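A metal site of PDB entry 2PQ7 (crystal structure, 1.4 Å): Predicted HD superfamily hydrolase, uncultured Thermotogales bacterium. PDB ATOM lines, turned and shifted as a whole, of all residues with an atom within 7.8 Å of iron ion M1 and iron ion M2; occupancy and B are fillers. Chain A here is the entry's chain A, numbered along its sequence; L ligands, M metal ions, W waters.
Water W1 binds iron ion M1 (2.1 Å). Iron ion M1 is bound by OD2 of Asp 67. Iron ion M1 is bound by OD1 of Asp 132 (2.1 Å). A ring nitrogen (NE2) of His 37 binds iron ion M1 (2.2 Å). Iron ion M1 is bound by a ring nitrogen (NE2) of His 66 (2.2 Å). An oxygen (O4) of LIG L1 is bound to iron ion M1 (2.2 Å). Iron ion M1 has six donor atoms within binding distance.
Four residues have an atom within 4 Å of iron ion M1: His 37, His 66, Asp 67 and Asp 132. The nearest printed residue that does not touch iron ion M1 is Val 41 (4.6 Å).
Iron ion M2 is bound by water W1 (2.0 Å), OD1 of Asp 67 (2.0 Å), O3 of LIG L1 (2.1 Å), O3 of LG2 L2 (2.1 Å), NE2 of His 112 (2.2 Å) and NE2 of His 80 (2.2 Å).
ND1 of His 112 is in hydrogen-bond range of O of Ile 109. A ring nitrogen (ND1) of His 37 sits at hydrogen-bond distance from the side-chain carboxylate (OD2) of Asp 135, at 2.8 Å. A ring nitrogen (ND1) of His 80 lies within hydrogen-bond range of the side-chain carboxylate (OE1) of Glu 73 (2.7 Å). A ring nitrogen (ND1) of His 66 sits at hydrogen-bond distance from the backbone carbonyl oxygen of Ala 63, at 2.7 Å.
Four residues have an atom within 4 Å of iron ion M2: His 66, Asp 67, His 80 and His 112.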
ATOM      1  N   ALA A  32      15.367 -12.393  23.518  1.00  0.00           N
ATOM      2  CA  ALA A  32      16.466 -11.742  22.844  1.00  0.00           C
ATOM      3  C   ALA A  32      17.750 -11.679  23.719  1.00  0.00           C
ATOM      4  O   ALA A  32      18.852 -11.424  23.209  1.00  0.00           O
ATOM      5  CB  ALA A  32      16.035 -10.324  22.461  1.00  0.00           C
ATOM      6  N   HIS A  33      17.618 -11.913  25.019  1.00  0.00           N
ATOM      7  CA  HIS A  33      18.746 -11.727  25.920  1.00  0.00           C
ATOM      8  C   HIS A  33      18.807 -12.717  27.057  1.00  0.00           C
ATOM      9  O   HIS A  33      19.480 -12.438  28.042  1.00  0.00           O
ATOM     10  CB  HIS A  33      18.645 -10.335  26.557  1.00  0.00           C
ATOM     11  CG  HIS A  33      18.559  -9.226  25.571  1.00  0.00           C
ATOM     12  ND1 HIS A  33      19.642  -8.785  24.849  1.00  0.00           N
ATOM     13  CD2 HIS A  33      17.516  -8.451  25.196  1.00  0.00           C
ATOM     14  CE1 HIS A  33      19.277  -7.796  24.063  1.00  0.00           C
ATOM     15  NE2 HIS A  33      17.985  -7.567  24.253  1.00  0.00           N
ATOM     16  N   ASP A  34      18.121 -13.849  26.941  1.00  0.00           N
ATOM     17  CA  ASP A  34      18.058 -14.790  28.052  1.00  0.00           C
ATOM     18  C   ASP A  34      19.348 -15.579  28.216  1.00  0.00           C
ATOM     19  O   ASP A  34      20.288 -15.458  27.425  1.00  0.00           O
ATOM     20  CB  ASP A  34      16.822 -15.694  27.914  1.00  0.00           C
ATOM     21  CG  ASP A  34      16.885 -16.629  26.722  1.00  0.00           C
ATOM     22  OD1 ASP A  34      17.976 -16.866  26.151  1.00  0.00           O
ATOM     23  OD2 ASP A  34      15.817 -17.109  26.327  1.00  0.00           O
ATOM     24  N   HIS A  37      21.371 -17.468  25.346  1.00  0.00           N
ATOM     25  CA  HIS A  37      22.332 -16.675  24.576  1.00  0.00           C
ATOM     26  C   HIS A  37      23.765 -16.798  25.171  1.00  0.00           C
ATOM     27  O   HIS A  37      24.747 -17.091  24.471  1.00  0.00           O
ATOM     28  CB  HIS A  37      21.891 -15.229  24.464  1.00  0.00           C
ATOM     29  CG  HIS A  37      22.988 -14.303  24.076  1.00  0.00           C
ATOM     30  ND1 HIS A  37      23.475 -14.206  22.779  1.00  0.00           N
ATOM     31  CD2 HIS A  37      23.756 -13.471  24.825  1.00  0.00           C
ATOM     32  CE1 HIS A  37      24.433 -13.292  22.746  1.00  0.00           C
ATOM     33  NE2 HIS A  37      24.623 -12.830  23.981  1.00  0.00           N
ATOM     34  N   THR A  38      23.890 -16.599  26.480  1.00  0.00           N
ATOM     35  CA  THR A  38      25.195 -16.702  27.144  1.00  0.00           C
ATOM     36  C   THR A  38      25.844 -18.054  26.919  1.00  0.00           C
ATOM     37  O   THR A  38      27.028 -18.173  26.622  1.00  0.00           O
ATOM     38  CB  THR A  38      25.056 -16.382  28.649  1.00  0.00           C
ATOM     39  OG1 THR A  38      24.841 -14.951  28.764  1.00  0.00           O
ATOM     40  CG2 THR A  38      26.272 -16.688  29.340  1.00  0.00           C
ATOM     41  N   VAL A  41      27.056 -18.216  23.340  1.00  0.00           N
ATOM     42  CA  VAL A  41      28.268 -17.366  23.197  1.00  0.00           C
ATOM     43  C   VAL A  41      29.488 -18.096  23.774  1.00  0.00           C
ATOM     44  O   VAL A  41      30.578 -18.100  23.200  1.00  0.00           O
ATOM     45  CB  VAL A  41      28.054 -15.973  23.799  1.00  0.00           C
ATOM     46  CG1 VAL A  41      29.384 -15.131  23.752  1.00  0.00           C
ATOM     47  CG2 VAL A  41      26.996 -15.242  23.018  1.00  0.00           C
ATOM     48  N   ALA A  63      32.979 -14.873  28.200  1.00  0.00           N
ATOM     49  CA  ALA A  63      31.695 -15.196  27.606  1.00  0.00           C
ATOM     50  C   ALA A  63      30.611 -15.462  28.640  1.00  0.00           C
ATOM     51  O   ALA A  63      29.489 -15.023  28.497  1.00  0.00           O
ATOM     52  CB  ALA A  63      31.831 -16.388  26.698  1.00  0.00           C
ATOM     53  N   HIS A  66      29.782 -12.051  30.331  1.00  0.00           N
ATOM     54  CA  HIS A  66      29.679 -10.786  29.567  1.00  0.00           C
ATOM     55  C   HIS A  66      28.320 -10.095  29.660  1.00  0.00           C
ATOM     56  O   HIS A  66      28.264  -8.900  29.685  1.00  0.00           O
ATOM     57  CB  HIS A  66      30.097 -10.956  28.109  1.00  0.00           C
ATOM     58  CG  HIS A  66      29.027 -11.479  27.205  1.00  0.00           C
ATOM     59  ND1 HIS A  66      28.582 -12.778  27.242  1.00  0.00           N
ATOM     60  CD2 HIS A  66      28.315 -10.857  26.236  1.00  0.00           C
ATOM     61  CE1 HIS A  66      27.622 -12.935  26.342  1.00  0.00           C
ATOM     62  NE2 HIS A  66      27.442 -11.776  25.711  1.00  0.00           N
ATOM     63  N   ASP A  67      27.244 -10.870  29.738  1.00  0.00           N
ATOM     64  CA  ASP A  67      25.905 -10.324  29.870  1.00  0.00           C
ATOM     65  C   ASP A  67      25.266 -10.580  31.260  1.00  0.00           C
ATOM     66  O   ASP A  67      24.043 -10.494  31.381  1.00  0.00           O
ATOM     67  CB  ASP A  67      25.029 -10.912  28.788  1.00  0.00           C
ATOM     68  CG  ASP A  67      25.249 -10.261  27.418  1.00  0.00           C
ATOM     69  OD1 ASP A  67      25.764  -9.115  27.272  1.00  0.00           O
ATOM     70  OD2 ASP A  67      24.842 -10.904  26.411  1.00  0.00           O
ATOM     71  N   ILE A  68      26.106 -10.828  32.284  1.00  0.00           N
ATOM     72  CA  ILE A  68      25.574 -11.164  33.598  1.00  0.00           C
ATOM     73  C   ILE A  68      24.798  -9.999  34.210  1.00  0.00           C
ATOM     74  O   ILE A  68      23.885 -10.226  34.994  1.00  0.00           O
ATOM     75  CB  ILE A  68      26.633 -11.728  34.533  1.00  0.00           C
ATOM     76  CG1 ILE A  68      25.967 -12.591  35.644  1.00  0.00           C
ATOM     77  CG2 ILE A  68      27.541 -10.631  35.131  1.00  0.00           C
ATOM     78  CD1 ILE A  68      26.912 -13.174  36.637  1.00  0.00           C
ATOM     79  N   ARG A  70      22.909  -8.001  32.312  1.00  0.00           N
ATOM     80  CA  ARG A  70      21.781  -7.674  31.415  1.00  0.00           C
ATOM     81  C   ARG A  70      20.458  -7.551  32.172  1.00  0.00           C
ATOM     82  O   ARG A  70      19.698  -6.623  31.947  1.00  0.00           O
ATOM     83  CB  ARG A  70      21.632  -8.681  30.260  1.00  0.00           C
ATOM     84  CG  ARG A  70      22.212  -8.253  28.982  1.00  0.00           C
ATOM     85  CD  ARG A  70      21.323  -7.248  28.327  1.00  0.00           C
ATOM     86  NE  ARG A  70      21.839  -6.852  27.025  1.00  0.00           N
ATOM     87  CZ  ARG A  70      21.315  -5.894  26.284  1.00  0.00           C
ATOM     88  NH1 ARG A  70      20.260  -5.212  26.710  1.00  0.00           N
ATOM     89  NH2 ARG A  70      21.860  -5.592  25.104  1.00  0.00           N
ATOM     90  N   GLU A  73      20.456  -4.323  33.859  1.00  0.00           N
ATOM     91  CA  GLU A  73      20.224  -3.182  32.930  1.00  0.00           C
ATOM     92  C   GLU A  73      18.723  -3.052  32.629  1.00  0.00           C
ATOM     93  O   GLU A  73      18.218  -1.942  32.552  1.00  0.00           O
ATOM     94  CB  GLU A  73      20.993  -3.378  31.621  1.00  0.00           C
ATOM     95  CG  GLU A  73      20.768  -2.225  30.660  1.00  0.00           C
ATOM     96  CD  GLU A  73      21.589  -2.275  29.397  1.00  0.00           C
ATOM     97  OE1 GLU A  73      22.700  -2.785  29.419  1.00  0.00           O
ATOM     98  OE2 GLU A  73      21.122  -1.754  28.378  1.00  0.00           O
ATOM     99  N   ASP A  79      24.304   0.584  32.086  1.00  0.00           N
ATOM    100  CA  ASP A  79      24.926  -0.166  31.005  1.00  0.00           C
ATOM    101  C   ASP A  79      25.546  -1.514  31.488  1.00  0.00           C
ATOM    102  O   ASP A  79      26.427  -1.496  32.341  1.00  0.00           O
ATOM    103  CB  ASP A  79      26.027   0.651  30.353  1.00  0.00           C
ATOM    104  CG  ASP A  79      26.913  -0.159  29.404  1.00  0.00           C
ATOM    105  OD1 ASP A  79      26.456  -0.976  28.586  1.00  0.00           O
ATOM    106  OD2 ASP A  79      28.132   0.037  29.464  1.00  0.00           O
ATOM    107  N   HIS A  80      25.092  -2.602  30.911  1.00  0.00           N
ATOM    108  CA  HIS A  80      25.511  -3.929  31.342  1.00  0.00           C
ATOM    109  C   HIS A  80      27.006  -4.232  31.073  1.00  0.00           C
ATOM    110  O   HIS A  80      27.634  -5.045  31.788  1.00  0.00           O
ATOM    111  CB  HIS A  80      24.635  -5.029  30.770  1.00  0.00           C
ATOM    112  CG  HIS A  80      24.853  -5.355  29.329  1.00  0.00           C
ATOM    113  ND1 HIS A  80      24.347  -4.583  28.286  1.00  0.00           N
ATOM    114  CD2 HIS A  80      25.505  -6.383  28.740  1.00  0.00           C
ATOM    115  CE1 HIS A  80      24.692  -5.126  27.136  1.00  0.00           C
ATOM    116  NE2 HIS A  80      25.376  -6.233  27.376  1.00  0.00           N
ATOM    117  N   ALA A  81      27.574  -3.610  30.050  1.00  0.00           N
ATOM    118  CA  ALA A  81      28.995  -3.833  29.764  1.00  0.00           C
ATOM    119  C   ALA A  81      29.859  -3.240  30.895  1.00  0.00           C
ATOM    120  O   ALA A  81      30.824  -3.859  31.385  1.00  0.00           O
ATOM    121  CB  ALA A  81      29.343  -3.228  28.390  1.00  0.00           C
ATOM    122  N   ILE A 109      34.854  -7.543  28.719  1.00  0.00           N
ATOM    123  CA  ILE A 109      33.436  -7.369  28.938  1.00  0.00           C
ATOM    124  C   ILE A 109      33.057  -5.917  28.747  1.00  0.00           C
ATOM    125  O   ILE A 109      32.038  -5.560  28.177  1.00  0.00           O
ATOM    126  CB  ILE A 109      33.062  -7.849  30.358  1.00  0.00           C
ATOM    127  CG1 ILE A 109      33.293  -9.378  30.466  1.00  0.00           C
ATOM    128  CG2 ILE A 109      31.601  -7.442  30.740  1.00  0.00           C
ATOM    129  CD1 ILE A 109      33.196  -9.922  31.887  1.00  0.00           C
ATOM    130  N   HIS A 112      32.646  -5.081  24.968  1.00  0.00           N
ATOM    131  CA  HIS A 112      31.909  -5.950  24.063  1.00  0.00           C
ATOM    132  C   HIS A 112      30.775  -5.424  23.192  1.00  0.00           C
ATOM    133  O   HIS A 112      30.482  -6.043  22.192  1.00  0.00           O
ATOM    134  CB  HIS A 112      31.474  -7.253  24.774  1.00  0.00           C
ATOM    135  CG  HIS A 112      30.144  -7.185  25.473  1.00  0.00           C
ATOM    136  ND1 HIS A 112      30.004  -6.837  26.794  1.00  0.00           N
ATOM    137  CD2 HIS A 112      28.900  -7.481  25.027  1.00  0.00           C
ATOM    138  CE1 HIS A 112      28.722  -6.895  27.126  1.00  0.00           C
ATOM    139  NE2 HIS A 112      28.029  -7.292  26.069  1.00  0.00           N
ATOM    140  N   ARG A 113      30.183  -4.304  23.569  1.00  0.00           N
ATOM    141  CA  ARG A 113      29.106  -3.746  22.716  1.00  0.00           C
ATOM    142  C   ARG A 113      29.642  -3.032  21.470  1.00  0.00           C
ATOM    143  O   ARG A 113      30.756  -2.490  21.521  1.00  0.00           O
ATOM    144  CB  ARG A 113      28.233  -2.766  23.467  1.00  0.00           C
ATOM    145  CG  ARG A 113      27.550  -3.254  24.690  1.00  0.00           C
ATOM    146  CD  ARG A 113      26.074  -2.801  24.598  1.00  0.00           C
ATOM    147  NE  ARG A 113      25.604  -2.055  25.746  1.00  0.00           N
ATOM    148  CZ  ARG A 113      24.319  -1.849  26.023  1.00  0.00           C
ATOM    149  NH1 ARG A 113      23.354  -2.357  25.252  1.00  0.00           N
ATOM    150  NH2 ARG A 113      23.995  -1.139  27.100  1.00  0.00           N
ATOM    151  N   LEU A 128      35.580 -12.467  22.296  1.00  0.00           N
ATOM    152  CA  LEU A 128      34.283 -12.312  22.952  1.00  0.00           C
ATOM    153  C   LEU A 128      33.308 -11.641  22.022  1.00  0.00           C
ATOM    154  O   LEU A 128      32.174 -12.094  21.880  1.00  0.00           O
ATOM    155  CB  LEU A 128      34.396 -11.507  24.245  1.00  0.00           C
ATOM    156  CG  LEU A 128      33.064 -11.190  24.915  1.00  0.00           C
ATOM    157  CD1 LEU A 128      32.272 -12.473  25.274  1.00  0.00           C
ATOM    158  CD2 LEU A 128      33.276 -10.343  26.137  1.00  0.00           C
ATOM    159  N   ALA A 131      32.296 -14.000  19.264  1.00  0.00           N
ATOM    160  CA  ALA A 131      31.444 -15.048  19.814  1.00  0.00           C
ATOM    161  C   ALA A 131      30.003 -14.560  20.073  1.00  0.00           C
ATOM    162  O   ALA A 131      29.014 -15.280  19.826  1.00  0.00           O
ATOM    163  CB  ALA A 131      32.057 -15.563  21.101  1.00  0.00           C
ATOM    164  N   ASP A 132      29.911 -13.328  20.548  1.00  0.00           N
ATOM    165  CA  ASP A 132      28.628 -12.678  20.853  1.00  0.00           C
ATOM    166  C   ASP A 132      27.895 -12.425  19.541  1.00  0.00           C
ATOM    167  O   ASP A 132      26.727 -12.821  19.375  1.00  0.00           O
ATOM    168  CB  ASP A 132      28.905 -11.378  21.577  1.00  0.00           C
ATOM    169  CG  ASP A 132      27.657 -10.705  22.142  1.00  0.00           C
ATOM    170  OD1 ASP A 132      26.785 -11.436  22.702  1.00  0.00           O
ATOM    171  OD2 ASP A 132      27.573  -9.469  22.045  1.00  0.00           O
ATOM    172  N   ARG A 133      28.601 -11.812  18.587  1.00  0.00           N
ATOM    173  CA  ARG A 133      27.930 -11.417  17.350  1.00  0.00           C
ATOM    174  C   ARG A 133      27.568 -12.592  16.486  1.00  0.00           C
ATOM    175  O   ARG A 133      26.551 -12.540  15.762  1.00  0.00           O
ATOM    176  CB  ARG A 133      28.746 -10.385  16.568  1.00  0.00           C
ATOM    177  CG  ARG A 133      28.943  -9.098  17.321  1.00  0.00           C
ATOM    178  CD  ARG A 133      29.896  -8.130  16.688  1.00  0.00           C
ATOM    179  NE  ARG A 133      29.395  -7.738  15.373  1.00  0.00           N
ATOM    180  CZ  ARG A 133      29.827  -8.175  14.185  1.00  0.00           C
ATOM    181  NH1 ARG A 133      30.883  -8.986  14.050  1.00  0.00           N
ATOM    182  NH2 ARG A 133      29.219  -7.730  13.091  1.00  0.00           N
ATOM    183  N   ASP A 135      26.066 -15.079  17.355  1.00  0.00           N
ATOM    184  CA  ASP A 135      24.754 -15.570  17.800  1.00  0.00           C
ATOM    185  C   ASP A 135      23.575 -14.960  17.044  1.00  0.00           C
ATOM    186  O   ASP A 135      22.461 -15.445  17.175  1.00  0.00           O
ATOM    187  CB  ASP A 135      24.587 -15.389  19.318  1.00  0.00           C
ATOM    188  CG  ASP A 135      23.490 -16.294  19.876  1.00  0.00           C
ATOM    189  OD1 ASP A 135      23.520 -17.516  19.586  1.00  0.00           O
ATOM    190  OD2 ASP A 135      22.649 -15.764  20.609  1.00  0.00           O
HETATM  191  P1  LIG L   1      23.140  -8.929  24.367  1.00  0.00           P
HETATM  192  O1  LIG L   1      22.467  -8.053  23.347  1.00  0.00           O
HETATM  193  O2  LIG L   1      22.025  -9.660  25.134  1.00  0.00           O
HETATM  194  O3  LIG L   1      23.895  -8.017  25.335  1.00  0.00           O
HETATM  195  O4  LIG L   1      23.925 -10.018  23.640  1.00  0.00           O
HETATM  196  P1  LG2 L   2      25.208  -5.995  23.086  1.00  0.00           P
HETATM  197  O1  LG2 L   2      23.860  -5.278  23.209  1.00  0.00           O
HETATM  198  O2  LG2 L   2      25.040  -7.323  22.375  1.00  0.00           O
HETATM  199  O3  LG2 L   2      25.851  -6.201  24.447  1.00  0.00           O
HETATM  200  O4  LG2 L   2      26.098  -5.102  22.257  1.00  0.00           O
HETATM  201 FE    FE M   1      25.715 -11.045  24.500  1.00  0.00          FE
HETATM  202 FE    FE M   2      25.876  -7.739  25.823  1.00  0.00          FE
HETATM  203  O   HOH W   1      26.414  -9.092  24.458  1.00  0.00           O
